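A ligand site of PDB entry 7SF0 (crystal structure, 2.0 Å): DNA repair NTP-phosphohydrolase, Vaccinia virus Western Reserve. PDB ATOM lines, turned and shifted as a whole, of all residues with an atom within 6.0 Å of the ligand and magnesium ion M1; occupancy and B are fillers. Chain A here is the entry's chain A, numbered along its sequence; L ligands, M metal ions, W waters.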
ATOM      1  N   ARG A  15      13.489  10.568   6.596  1.00  0.00           N
ATOM      2  CA  ARG A  15      12.970  11.182   5.381  1.00  0.00           C
ATOM      3  C   ARG A  15      12.558  12.638   5.527  1.00  0.00           C
ATOM      4  O   ARG A  15      12.520  13.375   4.544  1.00  0.00           O
ATOM      5  CB  ARG A  15      11.758  10.398   4.873  1.00  0.00           C
ATOM      6  CG  ARG A  15      12.097   9.044   4.326  1.00  0.00           C
ATOM      7  CD  ARG A  15      11.141   8.706   3.220  1.00  0.00           C
ATOM      8  NE  ARG A  15       9.815   8.377   3.718  1.00  0.00           N
ATOM      9  CZ  ARG A  15       8.710   8.424   2.983  1.00  0.00           C
ATOM     10  NH1 ARG A  15       8.771   8.817   1.711  1.00  0.00           N
ATOM     11  NH2 ARG A  15       7.544   8.099   3.516  1.00  0.00           N
ATOM     12  N   GLU A  16      12.215  13.047   6.750  1.00  0.00           N
ATOM     13  CA  GLU A  16      11.634  14.359   6.974  1.00  0.00           C
ATOM     14  C   GLU A  16      12.240  15.087   8.155  1.00  0.00           C
ATOM     15  O   GLU A  16      12.737  14.475   9.100  1.00  0.00           O
ATOM     16  CB  GLU A  16      10.116  14.244   7.213  1.00  0.00           C
ATOM     17  CG  GLU A  16       9.319  13.716   6.027  1.00  0.00           C
ATOM     18  CD  GLU A  16       7.852  13.498   6.360  1.00  0.00           C
ATOM     19  OE1 GLU A  16       7.559  12.755   7.324  1.00  0.00           O
ATOM     20  OE2 GLU A  16       6.986  14.054   5.653  1.00  0.00           O
ATOM     21  N   ASP A  31      -2.916  28.653  -1.146  1.00  0.00           N
ATOM     22  CA  ASP A  31      -2.273  27.344  -1.078  1.00  0.00           C
ATOM     23  C   ASP A  31      -2.403  26.677   0.285  1.00  0.00           C
ATOM     24  O   ASP A  31      -1.579  25.839   0.655  1.00  0.00           O
ATOM     25  CB  ASP A  31      -0.796  27.487  -1.441  1.00  0.00           C
ATOM     26  CG  ASP A  31      -0.279  26.337  -2.279  1.00  0.00           C
ATOM     27  OD1 ASP A  31      -0.534  25.165  -1.920  1.00  0.00           O
ATOM     28  OD2 ASP A  31       0.384  26.597  -3.308  1.00  0.00           O
ATOM     29  N   HIS A  33      -3.210  24.246   3.146  1.00  0.00           N
ATOM     30  CA  HIS A  33      -3.635  22.921   3.590  1.00  0.00           C
ATOM     31  C   HIS A  33      -4.116  22.916   5.016  1.00  0.00           C
ATOM     32  O   HIS A  33      -3.391  23.334   5.919  1.00  0.00           O
ATOM     33  CB  HIS A  33      -2.503  21.879   3.571  1.00  0.00           C
ATOM     34  CG  HIS A  33      -2.220  21.292   2.222  1.00  0.00           C
ATOM     35  ND1 HIS A  33      -1.327  21.861   1.355  1.00  0.00           N
ATOM     36  CD2 HIS A  33      -2.783  20.247   1.573  1.00  0.00           C
ATOM     37  CE1 HIS A  33      -1.283  21.146   0.249  1.00  0.00           C
ATOM     38  NE2 HIS A  33      -2.190  20.182   0.331  1.00  0.00           N
ATOM     39  N   PHE A  35      -5.162  20.146   7.840  1.00  0.00           N
ATOM     40  CA  PHE A  35      -5.166  18.770   8.311  1.00  0.00           C
ATOM     41  C   PHE A  35      -6.078  18.611   9.516  1.00  0.00           C
ATOM     42  O   PHE A  35      -6.104  19.454  10.430  1.00  0.00           O
ATOM     43  CB  PHE A  35      -3.763  18.314   8.705  1.00  0.00           C
ATOM     44  CG  PHE A  35      -2.780  18.251   7.574  1.00  0.00           C
ATOM     45  CD1 PHE A  35      -2.754  17.160   6.717  1.00  0.00           C
ATOM     46  CD2 PHE A  35      -1.853  19.254   7.397  1.00  0.00           C
ATOM     47  CE1 PHE A  35      -1.840  17.093   5.679  1.00  0.00           C
ATOM     48  CE2 PHE A  35      -0.930  19.208   6.368  1.00  0.00           C
ATOM     49  CZ  PHE A  35      -0.923  18.125   5.505  1.00  0.00           C
ATOM     50  N   ARG A  50      -1.770   6.982   2.598  1.00  0.00           N
ATOM     51  CA  ARG A  50      -1.960   7.620   1.298  1.00  0.00           C
ATOM     52  C   ARG A  50      -2.055   6.554   0.217  1.00  0.00           C
ATOM     53  O   ARG A  50      -1.352   5.544   0.276  1.00  0.00           O
ATOM     54  CB  ARG A  50      -0.813   8.592   1.016  1.00  0.00           C
ATOM     55  CG  ARG A  50      -1.092   9.639  -0.059  1.00  0.00           C
ATOM     56  CD  ARG A  50       0.095  10.581  -0.138  1.00  0.00           C
ATOM     57  NE  ARG A  50      -0.132  11.763  -0.964  1.00  0.00           N
ATOM     58  CZ  ARG A  50       0.360  11.937  -2.178  1.00  0.00           C
ATOM     59  NH1 ARG A  50       1.098  10.984  -2.740  1.00  0.00           N
ATOM     60  NH2 ARG A  50       0.103  13.052  -2.847  1.00  0.00           N
ATOM     61  N   PHE A  54       4.609   9.047  -1.623  1.00  0.00           N
ATOM     62  CA  PHE A  54       5.324  10.233  -2.098  1.00  0.00           C
ATOM     63  C   PHE A  54       6.438   9.825  -3.070  1.00  0.00           C
ATOM     64  O   PHE A  54       6.680  10.495  -4.077  1.00  0.00           O
ATOM     65  CB  PHE A  54       5.930  11.005  -0.926  1.00  0.00           C
ATOM     66  CG  PHE A  54       4.904  11.602   0.010  1.00  0.00           C
ATOM     67  CD1 PHE A  54       3.700  12.076  -0.477  1.00  0.00           C
ATOM     68  CD2 PHE A  54       5.153  11.691   1.370  1.00  0.00           C
ATOM     69  CE1 PHE A  54       2.765  12.625   0.382  1.00  0.00           C
ATOM     70  CE2 PHE A  54       4.217  12.240   2.228  1.00  0.00           C
ATOM     71  CZ  PHE A  54       3.023  12.707   1.734  1.00  0.00           C
ATOM     72  N   ALA A  55       7.112   8.730  -2.750  1.00  0.00           N
ATOM     73  CA  ALA A  55       8.218   8.240  -3.567  1.00  0.00           C
ATOM     74  C   ALA A  55       7.760   7.909  -4.989  1.00  0.00           C
ATOM     75  O   ALA A  55       8.403   8.311  -5.952  1.00  0.00           O
ATOM     76  CB  ALA A  55       8.865   7.020  -2.906  1.00  0.00           C
ATOM     77  N   GLN A  57       4.977   8.862  -6.578  1.00  0.00           N
ATOM     78  CA  GLN A  57       4.501  10.087  -7.219  1.00  0.00           C
ATOM     79  C   GLN A  57       5.686  10.840  -7.825  1.00  0.00           C
ATOM     80  O   GLN A  57       5.667  11.223  -9.012  1.00  0.00           O
ATOM     81  CB  GLN A  57       3.756  10.969  -6.217  1.00  0.00           C
ATOM     82  CG  GLN A  57       3.349  12.326  -6.773  1.00  0.00           C
ATOM     83  CD  GLN A  57       2.504  13.131  -5.786  1.00  0.00           C
ATOM     84  OE1 GLN A  57       1.680  12.586  -5.067  1.00  0.00           O
ATOM     85  NE2 GLN A  57       2.722  14.439  -5.768  1.00  0.00           N
ATOM     86  N   ALA A  58       6.720  11.048  -7.011  1.00  0.00           N
ATOM     87  CA  ALA A  58       7.926  11.713  -7.470  1.00  0.00           C
ATOM     88  C   ALA A  58       8.560  10.980  -8.653  1.00  0.00           C
ATOM     89  O   ALA A  58       8.882  11.595  -9.682  1.00  0.00           O
ATOM     90  CB  ALA A  58       8.913  11.835  -6.332  1.00  0.00           C
ATOM     91  N   ILE A 107      -0.430   9.713   6.641  1.00  0.00           N
ATOM     92  CA  ILE A 107      -0.773  11.123   6.504  1.00  0.00           C
ATOM     93  C   ILE A 107      -1.988  11.475   7.342  1.00  0.00           C
ATOM     94  O   ILE A 107      -2.896  10.664   7.520  1.00  0.00           O
ATOM     95  CB  ILE A 107      -1.063  11.518   5.028  1.00  0.00           C
ATOM     96  CG1 ILE A 107      -2.175  10.630   4.437  1.00  0.00           C
ATOM     97  CG2 ILE A 107       0.191  11.439   4.164  1.00  0.00           C
ATOM     98  CD1 ILE A 107      -2.685  11.142   3.111  1.00  0.00           C
ATOM     99  N   LYS A 112      -6.850  20.980   0.652  1.00  0.00           N
ATOM    100  CA  LYS A 112      -6.826  22.384   0.198  1.00  0.00           C
ATOM    101  C   LYS A 112      -8.014  23.211   0.734  1.00  0.00           C
ATOM    102  O   LYS A 112      -9.163  22.797   0.673  1.00  0.00           O
ATOM    103  CB  LYS A 112      -6.836  22.431  -1.348  1.00  0.00           C
ATOM    104  CG  LYS A 112      -5.480  22.324  -2.087  1.00  0.00           C
ATOM    105  CD  LYS A 112      -4.418  23.232  -1.486  1.00  0.00           C
ATOM    106  CE  LYS A 112      -3.048  22.646  -1.704  1.00  0.00           C
ATOM    107  NZ  LYS A 112      -2.926  22.083  -3.071  1.00  0.00           N
ATOM    108  N   THR A 149       7.330  21.216   6.889  1.00  0.00           N
ATOM    109  CA  THR A 149       8.050  19.976   6.595  1.00  0.00           C
ATOM    110  C   THR A 149       9.103  20.129   5.509  1.00  0.00           C
ATOM    111  O   THR A 149       8.805  20.601   4.419  1.00  0.00           O
ATOM    112  CB  THR A 149       7.070  18.859   6.147  1.00  0.00           C
ATOM    113  OG1 THR A 149       6.006  18.728   7.100  1.00  0.00           O
ATOM    114  CG2 THR A 149       7.802  17.522   6.019  1.00  0.00           C
ATOM    115  N   ARG A 150      10.336  19.742   5.799  1.00  0.00           N
ATOM    116  CA  ARG A 150      11.330  19.562   4.761  1.00  0.00           C
ATOM    117  C   ARG A 150      11.460  18.084   4.429  1.00  0.00           C
ATOM    118  O   ARG A 150      11.728  17.266   5.310  1.00  0.00           O
ATOM    119  CB  ARG A 150      12.701  20.121   5.178  1.00  0.00           C
ATOM    120  CG  ARG A 150      13.816  19.711   4.221  1.00  0.00           C
ATOM    121  CD  ARG A 150      15.116  20.461   4.461  1.00  0.00           C
ATOM    122  NE  ARG A 150      14.981  21.881   4.174  1.00  0.00           N
ATOM    123  CZ  ARG A 150      15.103  22.411   2.959  1.00  0.00           C
ATOM    124  NH1 ARG A 150      15.357  21.632   1.916  1.00  0.00           N
ATOM    125  NH2 ARG A 150      14.959  23.724   2.796  1.00  0.00           N
ATOM    126  N   ASP A 151      11.243  17.742   3.168  1.00  0.00           N
ATOM    127  CA  ASP A 151      11.502  16.395   2.693  1.00  0.00           C
ATOM    128  C   ASP A 151      12.991  16.298   2.366  1.00  0.00           C
ATOM    129  O   ASP A 151      13.484  17.016   1.498  1.00  0.00           O
ATOM    130  CB  ASP A 151      10.645  16.055   1.472  1.00  0.00           C
ATOM    131  CG  ASP A 151      10.795  14.604   1.029  1.00  0.00           C
ATOM    132  OD1 ASP A 151      11.934  14.182   0.746  1.00  0.00           O
ATOM    133  OD2 ASP A 151       9.776  13.880   0.997  1.00  0.00           O
ATOM    134  N   PHE A 154      13.829  14.846  -1.390  1.00  0.00           N
ATOM    135  CA  PHE A 154      13.520  15.615  -2.589  1.00  0.00           C
ATOM    136  C   PHE A 154      13.878  17.094  -2.452  1.00  0.00           C
ATOM    137  O   PHE A 154      13.780  17.844  -3.420  1.00  0.00           O
ATOM    138  CB  PHE A 154      12.038  15.460  -2.931  1.00  0.00           C
ATOM    139  CG  PHE A 154      11.620  14.037  -3.125  1.00  0.00           C
ATOM    140  CD1 PHE A 154      12.366  13.181  -3.918  1.00  0.00           C
ATOM    141  CD2 PHE A 154      10.495  13.536  -2.491  1.00  0.00           C
ATOM    142  CE1 PHE A 154      11.998  11.856  -4.101  1.00  0.00           C
ATOM    143  CE2 PHE A 154      10.116  12.210  -2.660  1.00  0.00           C
ATOM    144  CZ  PHE A 154      10.863  11.370  -3.465  1.00  0.00           C
ATOM    145  N   TYR A 158       7.181  22.134   2.682  1.00  0.00           N
ATOM    146  CA  TYR A 158       5.721  22.207   2.643  1.00  0.00           C
ATOM    147  C   TYR A 158       5.188  22.881   3.911  1.00  0.00           C
ATOM    148  O   TYR A 158       5.755  22.710   4.991  1.00  0.00           O
ATOM    149  CB  TYR A 158       5.103  20.812   2.517  1.00  0.00           C
ATOM    150  CG  TYR A 158       5.617  19.997   1.361  1.00  0.00           C
ATOM    151  CD1 TYR A 158       6.759  19.209   1.485  1.00  0.00           C
ATOM    152  CD2 TYR A 158       4.959  19.992   0.141  1.00  0.00           C
ATOM    153  CE1 TYR A 158       7.224  18.454   0.422  1.00  0.00           C
ATOM    154  CE2 TYR A 158       5.414  19.238  -0.922  1.00  0.00           C
ATOM    155  CZ  TYR A 158       6.546  18.476  -0.781  1.00  0.00           C
ATOM    156  OH  TYR A 158       7.001  17.736  -1.843  1.00  0.00           O
ATOM    157  N   ILE A 159       4.095  23.621   3.774  1.00  0.00           N
ATOM    158  CA  ILE A 159       3.421  24.230   4.930  1.00  0.00           C
ATOM    159  C   ILE A 159       2.003  23.694   5.056  1.00  0.00           C
ATOM    160  O   ILE A 159       1.297  23.578   4.066  1.00  0.00           O
ATOM    161  CB  ILE A 159       3.358  25.773   4.813  1.00  0.00           C
ATOM    162  CG1 ILE A 159       4.724  26.367   4.487  1.00  0.00           C
ATOM    163  CG2 ILE A 159       2.815  26.372   6.116  1.00  0.00           C
ATOM    164  CD1 ILE A 159       5.702  26.304   5.619  1.00  0.00           C
ATOM    165  N   GLY A 160       1.592  23.385   6.276  1.00  0.00           N
ATOM    166  CA  GLY A 160       0.214  22.979   6.517  1.00  0.00           C
ATOM    167  C   GLY A 160      -0.238  23.434   7.895  1.00  0.00           C
ATOM    168  O   GLY A 160       0.576  23.857   8.692  1.00  0.00           O
ATOM    169  N   GLU A 183      -7.430   9.117  -2.937  1.00  0.00           N
ATOM    170  CA  GLU A 183      -6.446   9.784  -2.092  1.00  0.00           C
ATOM    171  C   GLU A 183      -5.947   8.908  -0.950  1.00  0.00           C
ATOM    172  O   GLU A 183      -4.794   9.019  -0.532  1.00  0.00           O
ATOM    173  CB  GLU A 183      -7.025  11.080  -1.536  1.00  0.00           C
ATOM    174  CG  GLU A 183      -7.254  12.148  -2.616  1.00  0.00           C
ATOM    175  CD  GLU A 183      -7.613  13.513  -2.039  1.00  0.00           C
ATOM    176  OE1 GLU A 183      -7.469  14.507  -2.768  1.00  0.00           O
ATOM    177  OE2 GLU A 183      -8.035  13.572  -0.870  1.00  0.00           O
ATOM    178  N   LYS A 198       7.132   7.977  10.992  1.00  0.00           N
ATOM    179  CA  LYS A 198       6.402   9.192  11.319  1.00  0.00           C
ATOM    180  C   LYS A 198       5.690   9.137  12.670  1.00  0.00           C
ATOM    181  O   LYS A 198       5.121  10.132  13.121  1.00  0.00           O
ATOM    182  CB  LYS A 198       5.374   9.498  10.236  1.00  0.00           C
ATOM    183  CG  LYS A 198       5.975   9.671   8.843  1.00  0.00           C
ATOM    184  CD  LYS A 198       4.888   9.935   7.820  1.00  0.00           C
ATOM    185  CE  LYS A 198       5.449  10.003   6.407  1.00  0.00           C
ATOM    186  NZ  LYS A 198       4.362  10.276   5.428  1.00  0.00           N
HETATM  187  P1  LIG L   1       0.210  18.423  -1.706  1.00  0.00           P
HETATM  188  O1  LIG L   1       1.185  17.720  -2.646  1.00  0.00           O
HETATM  189  O2  LIG L   1       0.054  19.853  -2.141  1.00  0.00           O
HETATM  190  O3  LIG L   1      -1.229  17.687  -1.751  1.00  0.00           O
HETATM  191  O4  LIG L   1       0.760  18.384  -0.220  1.00  0.00           O
HETATM  192  P2  LIG L   1      -1.448  16.150  -2.073  1.00  0.00           P
HETATM  193  O5  LIG L   1      -0.760  15.306  -1.021  1.00  0.00           O
HETATM  194  O6  LIG L   1      -2.917  15.843  -2.077  1.00  0.00           O
HETATM  195  O7  LIG L   1      -0.876  15.848  -3.421  1.00  0.00           O
HETATM  196  C1  LIG L   1      -0.083  17.860   0.815  1.00  0.00           C
HETATM  197  C2  LIG L   1       0.695  17.640   1.945  1.00  0.00           C
HETATM  198  O8  LIG L   1       1.297  16.272   1.843  1.00  0.00           O
HETATM  199  C3  LIG L   1       1.953  18.634   1.978  1.00  0.00           C
HETATM  200  O9  LIG L   1       1.626  19.886   2.734  1.00  0.00           O
HETATM  201  C4  LIG L   1       2.828  17.979   2.560  1.00  0.00           C
HETATM  202  O10 LIG L   1       2.627  18.063   4.016  1.00  0.00           O
HETATM  203  C5  LIG L   1       2.588  16.415   2.107  1.00  0.00           C
HETATM  204  N1  LIG L   1       3.342  16.058   0.994  1.00  0.00           N
HETATM  205  C6  LIG L   1       2.943  16.080  -0.403  1.00  0.00           C
HETATM  206  N2  LIG L   1       4.099  15.573  -1.193  1.00  0.00           N
HETATM  207  C7  LIG L   1       4.140  15.438  -2.632  1.00  0.00           C
HETATM  208  C8  LIG L   1       5.116  15.277  -0.259  1.00  0.00           C
HETATM  209  C9  LIG L   1       6.505  14.725  -0.466  1.00  0.00           C
HETATM  210  O11 LIG L   1       6.929  14.476  -1.586  1.00  0.00           O
HETATM  211  N3  LIG L   1       7.333  14.514   0.658  1.00  0.00           N
HETATM  212  C10 LIG L   1       6.861  14.813   1.969  1.00  0.00           C
HETATM  213  N4  LIG L   1       7.688  14.595   3.084  1.00  0.00           N
HETATM  214  N5  LIG L   1       5.521  15.330   2.164  1.00  0.00           N
HETATM  215  C11 LIG L   1       4.673  15.557   1.028  1.00  0.00           C
HETATM  216 MG    MG M   1       0.756  16.161  -4.535  1.00  0.00          MG
HETATM  217 MG    MG M   2      -8.364  15.619  -0.031  1.00  0.00          MG
HETATM  218  O   HOH W   1       6.116  13.116  -3.976  1.00  0.00           O
HETATM  219  O   HOH W   2      -1.414  14.803   2.784  1.00  0.00           O
HETATM  220  O   HOH W   3       1.492  21.512  -0.503  1.00  0.00           O
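Water W3 lies within hydrogen-bond range of O2 of the ligand (2.7 Å) and ND1 of His 33 (3.4 Å).
Water W1 bridges O of Phe 54 and O11 of the ligand.
The side-chain carboxylate (OD2) of Asp 151 is in hydrogen-bond range of a nitrogen (N3) of the ligand (2.5 Å).
The side-chain carboxylate (OE2) of Glu 16 lies within hydrogen-bond range of a nitrogen (N4) of the ligand (2.7 Å).
O5 of the ligand lies within salt-bridge range of NH2 of Arg 50, at 3.0 Å.
An oxygen (O2) of the ligand lies close to a ring nitrogen (NE2) of His 33 (3.4 Å).
OH of Tyr 158 sits at hydrogen-bond distance from O11 of the ligand (3.3 Å).
An oxygen (O2) of the ligand is in salt-bridge range of the side-chain amino group (NZ) of Lys 112 (3.8 Å).
N of Phe 154 is in hydrogen-bond range of OD1 of Asp 151 (2.9 Å).
The guanidinium group (NH2) of Arg 50 lies within hydrogen-bond range of the side-chain amide oxygen (OE1) of Gln 57 (2.8 Å).
N of Tyr 158 lies within hydrogen-bond range of O of Thr 149 (2.8 Å).
Merely in contact with the ligand: Phe 35, Phe 54, Gln 57, Phe 154 and Ile 159.
Within 4 Å of the ligand: Glu 16, His 33, Phe 35, Arg 50, Phe 54, Gln 57, Lys 112, Asp 151, Phe 154, Tyr 158 and Ile 159.
The nearest printed residue that does not touch the ligand is Thr 149 (4.1 Å).
NH2 of Arg 50 touches magnesium ion M1 (3.6 Å).
Gln 57 touches magnesium ion M1.
Of the 21 residues printed, 2 come within 4 Å of magnesium ion M1.
The nearest printed residue that does not touch magnesium ion M1 is Phe 54 (6.4 Å).
Magnesium ion M1 is bound by an oxygen (O7) of the ligand and an oxygen (O1) of the ligand.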
